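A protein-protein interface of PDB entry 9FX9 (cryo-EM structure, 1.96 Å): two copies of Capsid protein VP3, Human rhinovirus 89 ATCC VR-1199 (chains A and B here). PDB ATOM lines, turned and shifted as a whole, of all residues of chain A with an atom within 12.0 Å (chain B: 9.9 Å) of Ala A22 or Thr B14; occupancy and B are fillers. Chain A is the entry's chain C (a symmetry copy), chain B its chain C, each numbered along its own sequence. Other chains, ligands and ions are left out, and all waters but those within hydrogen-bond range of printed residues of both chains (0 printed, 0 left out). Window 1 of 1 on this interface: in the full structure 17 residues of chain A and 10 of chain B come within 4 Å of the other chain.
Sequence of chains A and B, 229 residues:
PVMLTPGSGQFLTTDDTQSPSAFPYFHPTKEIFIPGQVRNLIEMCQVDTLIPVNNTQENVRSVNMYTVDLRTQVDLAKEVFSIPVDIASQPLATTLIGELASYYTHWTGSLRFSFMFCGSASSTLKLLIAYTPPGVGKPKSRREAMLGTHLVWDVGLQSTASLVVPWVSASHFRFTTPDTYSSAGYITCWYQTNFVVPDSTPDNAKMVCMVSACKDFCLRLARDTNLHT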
ATOM      1  N   GLN A  18     -11.785  12.385  14.037  1.00  0.00           N
ATOM      2  CA  GLN A  18     -11.653  12.113  15.469  1.00  0.00           C
ATOM      3  C   GLN A  18     -12.269  13.255  16.297  1.00  0.00           C
ATOM      4  O   GLN A  18     -12.459  14.372  15.808  1.00  0.00           O
ATOM      5  CB  GLN A  18     -10.181  11.881  15.832  1.00  0.00           C
ATOM      6  CG  GLN A  18      -9.633  10.604  15.174  1.00  0.00           C
ATOM      7  CD  GLN A  18      -8.178  10.316  15.532  1.00  0.00           C
ATOM      8  OE1 GLN A  18      -7.580  10.916  16.415  1.00  0.00           O
ATOM      9  NE2 GLN A  18      -7.539   9.390  14.851  1.00  0.00           N
ATOM     10  N   SER A  19     -12.581  12.985  17.559  1.00  0.00           N
ATOM     11  CA  SER A  19     -13.030  13.986  18.526  1.00  0.00           C
ATOM     12  C   SER A  19     -12.608  13.584  19.944  1.00  0.00           C
ATOM     13  O   SER A  19     -12.339  12.402  20.186  1.00  0.00           O
ATOM     14  CB  SER A  19     -14.541  14.204  18.424  1.00  0.00           C
ATOM     15  OG  SER A  19     -15.285  13.120  18.930  1.00  0.00           O
ATOM     16  N   PRO A  20     -12.500  14.531  20.889  1.00  0.00           N
ATOM     17  CA  PRO A  20     -12.006  14.219  22.220  1.00  0.00           C
ATOM     18  C   PRO A  20     -13.013  13.370  23.000  1.00  0.00           C
ATOM     19  O   PRO A  20     -14.219  13.623  22.981  1.00  0.00           O
ATOM     20  CB  PRO A  20     -11.725  15.570  22.882  1.00  0.00           C
ATOM     21  CG  PRO A  20     -12.690  16.517  22.178  1.00  0.00           C
ATOM     22  CD  PRO A  20     -12.750  15.958  20.761  1.00  0.00           C
ATOM     23  N   SER A  21     -12.518  12.373  23.729  1.00  0.00           N
ATOM     24  CA  SER A  21     -13.334  11.693  24.735  1.00  0.00           C
ATOM     25  C   SER A  21     -13.682  12.665  25.855  1.00  0.00           C
ATOM     26  O   SER A  21     -12.807  13.321  26.418  1.00  0.00           O
ATOM     27  CB  SER A  21     -12.622  10.460  25.291  1.00  0.00           C
ATOM     28  OG  SER A  21     -13.434   9.853  26.278  1.00  0.00           O
ATOM     29  N   ALA A  22     -14.962  12.764  26.192  1.00  0.00           N
ATOM     30  CA  ALA A  22     -15.433  13.549  27.327  1.00  0.00           C
ATOM     31  C   ALA A  22     -14.961  12.957  28.667  1.00  0.00           C
ATOM     32  O   ALA A  22     -14.860  13.682  29.653  1.00  0.00           O
ATOM     33  CB  ALA A  22     -16.958  13.610  27.232  1.00  0.00           C
ATOM     34  N   PHE A  23     -14.646  11.662  28.707  1.00  0.00           N
ATOM     35  CA  PHE A  23     -14.306  10.929  29.924  1.00  0.00           C
ATOM     36  C   PHE A  23     -13.099  10.016  29.682  1.00  0.00           C
ATOM     37  O   PHE A  23     -13.259   8.804  29.548  1.00  0.00           O
ATOM     38  CB  PHE A  23     -15.538  10.160  30.438  1.00  0.00           C
ATOM     39  CG  PHE A  23     -16.735  11.034  30.746  1.00  0.00           C
ATOM     40  CD1 PHE A  23     -16.889  11.597  32.024  1.00  0.00           C
ATOM     41  CD2 PHE A  23     -17.689  11.305  29.751  1.00  0.00           C
ATOM     42  CE1 PHE A  23     -17.990  12.423  32.299  1.00  0.00           C
ATOM     43  CE2 PHE A  23     -18.788  12.136  30.023  1.00  0.00           C
ATOM     44  CZ  PHE A  23     -18.940  12.694  31.303  1.00  0.00           C
ATOM     45  N   PRO A  24     -11.867  10.553  29.630  1.00  0.00           N
ATOM     46  CA  PRO A  24     -10.674   9.739  29.823  1.00  0.00           C
ATOM     47  C   PRO A  24     -10.667   9.187  31.260  1.00  0.00           C
ATOM     48  O   PRO A  24     -11.469   9.593  32.099  1.00  0.00           O
ATOM     49  CB  PRO A  24      -9.507  10.679  29.529  1.00  0.00           C
ATOM     50  CG  PRO A  24     -10.035  12.035  29.983  1.00  0.00           C
ATOM     51  CD  PRO A  24     -11.525  11.966  29.652  1.00  0.00           C
ATOM     52  N   TYR A  25      -9.785   8.238  31.557  1.00  0.00           N
ATOM     53  CA  TYR A  25      -9.768   7.446  32.801  1.00  0.00           C
ATOM     54  C   TYR A  25     -10.957   6.489  32.987  1.00  0.00           C
ATOM     55  O   TYR A  25     -10.778   5.413  33.562  1.00  0.00           O
ATOM     56  CB  TYR A  25      -9.584   8.320  34.056  1.00  0.00           C
ATOM     57  CG  TYR A  25      -8.513   9.390  33.970  1.00  0.00           C
ATOM     58  CD1 TYR A  25      -7.159   9.021  33.943  1.00  0.00           C
ATOM     59  CD2 TYR A  25      -8.874  10.748  33.964  1.00  0.00           C
ATOM     60  CE1 TYR A  25      -6.159  10.009  33.917  1.00  0.00           C
ATOM     61  CE2 TYR A  25      -7.877  11.741  33.941  1.00  0.00           C
ATOM     62  CZ  TYR A  25      -6.517  11.372  33.926  1.00  0.00           C
ATOM     63  OH  TYR A  25      -5.547  12.320  33.926  1.00  0.00           O
ATOM     64  N   PHE A  26     -12.149   6.807  32.485  1.00  0.00           N
ATOM     65  CA  PHE A  26     -13.275   5.874  32.475  1.00  0.00           C
ATOM     66  C   PHE A  26     -13.017   4.700  31.524  1.00  0.00           C
ATOM     67  O   PHE A  26     -12.736   4.895  30.342  1.00  0.00           O
ATOM     68  CB  PHE A  26     -14.573   6.599  32.105  1.00  0.00           C
ATOM     69  CG  PHE A  26     -15.775   5.679  32.052  1.00  0.00           C
ATOM     70  CD1 PHE A  26     -16.410   5.277  33.241  1.00  0.00           C
ATOM     71  CD2 PHE A  26     -16.242   5.187  30.823  1.00  0.00           C
ATOM     72  CE1 PHE A  26     -17.507   4.403  33.199  1.00  0.00           C
ATOM     73  CE2 PHE A  26     -17.351   4.329  30.779  1.00  0.00           C
ATOM     74  CZ  PHE A  26     -17.981   3.930  31.965  1.00  0.00           C
ATOM     75  N   HIS A  27     -13.146   3.480  32.030  1.00  0.00           N
ATOM     76  CA  HIS A  27     -13.091   2.262  31.225  1.00  0.00           C
ATOM     77  C   HIS A  27     -14.515   1.703  31.097  1.00  0.00           C
ATOM     78  O   HIS A  27     -15.106   1.344  32.115  1.00  0.00           O
ATOM     79  CB  HIS A  27     -12.133   1.257  31.879  1.00  0.00           C
ATOM     80  CG  HIS A  27     -10.686   1.682  31.834  1.00  0.00           C
ATOM     81  ND1 HIS A  27     -10.105   2.735  32.506  1.00  0.00           N
ATOM     82  CD2 HIS A  27      -9.715   1.140  31.038  1.00  0.00           C
ATOM     83  CE1 HIS A  27      -8.818   2.814  32.142  1.00  0.00           C
ATOM     84  NE2 HIS A  27      -8.528   1.855  31.245  1.00  0.00           N
ATOM     85  N   PRO A  28     -15.088   1.621  29.882  1.00  0.00           N
ATOM     86  CA  PRO A  28     -16.411   1.047  29.660  1.00  0.00           C
ATOM     87  C   PRO A  28     -16.543  -0.382  30.183  1.00  0.00           C
ATOM     88  O   PRO A  28     -15.575  -1.143  30.184  1.00  0.00           O
ATOM     89  CB  PRO A  28     -16.628   1.076  28.146  1.00  0.00           C
ATOM     90  CG  PRO A  28     -15.757   2.237  27.694  1.00  0.00           C
ATOM     91  CD  PRO A  28     -14.564   2.150  28.637  1.00  0.00           C
ATOM     92  N   GLN B  10     -12.745  24.639  21.254  1.00  0.00           N
ATOM     93  CA  GLN B  10     -13.451  24.286  22.486  1.00  0.00           C
ATOM     94  C   GLN B  10     -12.530  24.366  23.704  1.00  0.00           C
ATOM     95  O   GLN B  10     -11.381  23.932  23.646  1.00  0.00           O
ATOM     96  CB  GLN B  10     -13.945  22.831  22.447  1.00  0.00           C
ATOM     97  CG  GLN B  10     -15.196  22.595  21.609  1.00  0.00           C
ATOM     98  CD  GLN B  10     -15.568  21.116  21.556  1.00  0.00           C
ATOM     99  OE1 GLN B  10     -14.840  20.226  21.965  1.00  0.00           O
ATOM    100  NE2 GLN B  10     -16.733  20.793  21.048  1.00  0.00           N
ATOM    101  N   PHE B  11     -13.082  24.782  24.840  1.00  0.00           N
ATOM    102  CA  PHE B  11     -12.573  24.341  26.130  1.00  0.00           C
ATOM    103  C   PHE B  11     -13.457  23.200  26.646  1.00  0.00           C
ATOM    104  O   PHE B  11     -14.470  23.415  27.306  1.00  0.00           O
ATOM    105  CB  PHE B  11     -12.449  25.506  27.113  1.00  0.00           C
ATOM    106  CG  PHE B  11     -12.038  25.095  28.516  1.00  0.00           C
ATOM    107  CD1 PHE B  11     -11.104  24.066  28.752  1.00  0.00           C
ATOM    108  CD2 PHE B  11     -12.631  25.734  29.612  1.00  0.00           C
ATOM    109  CE1 PHE B  11     -10.781  23.686  30.065  1.00  0.00           C
ATOM    110  CE2 PHE B  11     -12.281  25.381  30.925  1.00  0.00           C
ATOM    111  CZ  PHE B  11     -11.358  24.356  31.153  1.00  0.00           C
ATOM    112  N   LEU B  12     -13.084  21.968  26.312  1.00  0.00           N
ATOM    113  CA  LEU B  12     -13.594  20.768  26.960  1.00  0.00           C
ATOM    114  C   LEU B  12     -12.850  20.595  28.289  1.00  0.00           C
ATOM    115  O   LEU B  12     -11.642  20.397  28.285  1.00  0.00           O
ATOM    116  CB  LEU B  12     -13.400  19.586  25.997  1.00  0.00           C
ATOM    117  CG  LEU B  12     -13.758  18.215  26.590  1.00  0.00           C
ATOM    118  CD1 LEU B  12     -15.231  18.145  26.970  1.00  0.00           C
ATOM    119  CD2 LEU B  12     -13.468  17.122  25.568  1.00  0.00           C
ATOM    120  N   THR B  13     -13.539  20.662  29.426  1.00  0.00           N
ATOM    121  CA  THR B  13     -12.885  20.637  30.750  1.00  0.00           C
ATOM    122  C   THR B  13     -12.130  19.338  31.042  1.00  0.00           C
ATOM    123  O   THR B  13     -11.211  19.337  31.855  1.00  0.00           O
ATOM    124  CB  THR B  13     -13.881  20.893  31.885  1.00  0.00           C
ATOM    125  OG1 THR B  13     -14.895  19.921  31.870  1.00  0.00           O
ATOM    126  CG2 THR B  13     -14.538  22.265  31.794  1.00  0.00           C
ATOM    127  N   THR B  14     -12.471  18.237  30.380  1.00  0.00           N
ATOM    128  CA  THR B  14     -11.791  16.942  30.489  1.00  0.00           C
ATOM    129  C   THR B  14     -10.705  16.716  29.429  1.00  0.00           C
ATOM    130  O   THR B  14     -10.212  15.596  29.307  1.00  0.00           O
ATOM    131  CB  THR B  14     -12.810  15.796  30.481  1.00  0.00           C
ATOM    132  OG1 THR B  14     -13.580  15.833  29.304  1.00  0.00           O
ATOM    133  CG2 THR B  14     -13.768  15.861  31.670  1.00  0.00           C
ATOM    134  N   ASP B  15     -10.302  17.729  28.652  1.00  0.00           N
ATOM    135  CA  ASP B  15      -9.239  17.578  27.652  1.00  0.00           C
ATOM    136  C   ASP B  15      -7.848  17.289  28.260  1.00  0.00           C
ATOM    137  O   ASP B  15      -7.603  17.438  29.456  1.00  0.00           O
ATOM    138  CB  ASP B  15      -9.212  18.750  26.651  1.00  0.00           C
ATOM    139  CG  ASP B  15      -8.681  20.107  27.148  1.00  0.00           C
ATOM    140  OD1 ASP B  15      -8.462  20.337  28.355  1.00  0.00           O
ATOM    141  OD2 ASP B  15      -8.420  20.978  26.291  1.00  0.00           O
ATOM    142  N   ASP B  16      -6.929  16.828  27.412  1.00  0.00           N
ATOM    143  CA  ASP B  16      -5.583  16.377  27.789  1.00  0.00           C
ATOM    144  C   ASP B  16      -4.533  16.821  26.753  1.00  0.00           C
ATOM    145  O   ASP B  16      -3.706  16.040  26.294  1.00  0.00           O
ATOM    146  CB  ASP B  16      -5.606  14.853  28.005  1.00  0.00           C
ATOM    147  CG  ASP B  16      -4.318  14.291  28.625  1.00  0.00           C
ATOM    148  OD1 ASP B  16      -3.597  15.033  29.317  1.00  0.00           O
ATOM    149  OD2 ASP B  16      -4.050  13.080  28.459  1.00  0.00           O
ATOM    150  N   THR B  17      -4.603  18.074  26.303  1.00  0.00           N
ATOM    151  CA  THR B  17      -3.610  18.635  25.372  1.00  0.00           C
ATOM    152  C   THR B  17      -2.339  19.047  26.114  1.00  0.00           C
ATOM    153  O   THR B  17      -2.359  19.316  27.313  1.00  0.00           O
ATOM    154  CB  THR B  17      -4.150  19.823  24.547  1.00  0.00           C
ATOM    155  OG1 THR B  17      -4.226  21.019  25.295  1.00  0.00           O
ATOM    156  CG2 THR B  17      -5.526  19.550  23.948  1.00  0.00           C
ATOM    157  N   LEU B 221     -16.326   5.255  37.376  1.00  0.00           N
ATOM    158  CA  LEU B 221     -17.115   6.432  37.050  1.00  0.00           C
ATOM    159  C   LEU B 221     -17.163   7.429  38.212  1.00  0.00           C
ATOM    160  O   LEU B 221     -18.107   7.446  38.997  1.00  0.00           O
ATOM    161  CB  LEU B 221     -18.479   5.991  36.486  1.00  0.00           C
ATOM    162  CG  LEU B 221     -19.381   7.139  36.017  1.00  0.00           C
ATOM    163  CD1 LEU B 221     -18.756   7.918  34.861  1.00  0.00           C
ATOM    164  CD2 LEU B 221     -20.719   6.569  35.549  1.00  0.00           C
ATOM    165  N   ALA B 222     -16.122   8.247  38.343  1.00  0.00           N
ATOM    166  CA  ALA B 222     -16.016   9.245  39.403  1.00  0.00           C
ATOM    167  C   ALA B 222     -17.190  10.239  39.402  1.00  0.00           C
ATOM    168  O   ALA B 222     -17.704  10.599  38.342  1.00  0.00           O
ATOM    169  CB  ALA B 222     -14.680   9.970  39.254  1.00  0.00           C
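OG1 of Thr B14 lies within hydrogen-bond range of O of Ala A22, 2.5 Å away.
Of chain B, only Thr B14 comes within 4 Å of Ala A22. Thr B14 touches just these residues of chain A: Ser A21, Ala A22 and Pro A24. Ser A21 touches just these residues of chain B: Leu B12 (3.95 Å) and Thr B14 (3.9 Å). No residue of chain B comes within 4 Å of Phe A23. Of chain A, only Pro A20 and Ser A21 come within 4 Å of Leu B12. No residue of chain A comes within 4 Å of Thr B13. No residue of chain A comes within 4 Å of Asp B16. Of the printed residues of chain A, Leu B221 touches Phe A26. Of the printed residues of chain B, Phe A26 touches Leu B221 (3.8 Å). Of the printed residues of chain B, Pro A20 touches Leu B12 (3.5 Å). His A27 touches none of the printed residues of chain B. The nearest residue of chain B that does not touch Ala A22 is Leu B12 (4.4 Å). The nearest residue of chain A that does not touch Thr B14 is Phe A23 (4.3 Å). The nearest printed residue of chain B that does not touch Pro A24 is Asp B16 (5.6 Å).
Of the 11 printed residues of chain A, 5 touch a printed residue of chain B. Hydrophobic or aromatic side chains of chain A that line the printed part of chain B: Pro A20, Pro A24 and Phe A26. Among the printed residues, 6 pairs touch across the chains. Among the printed residues, no Asp or Glu carboxylate lies within 4 Å of a Lys or Arg side-chain nitrogen of the other chain.
No position is printed for both chains.
Among the printed residues, merely in contact across the chains: Pro A20 with Leu B12, Ser A21 with Leu B12, Ser A21 with Thr B14, Pro A24 with Thr B14 and Phe A26 with Leu B221.
The side-chain hydroxyl of Ser A21 lies close to the backbone NH of Phe A23, 3.3 Å away.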
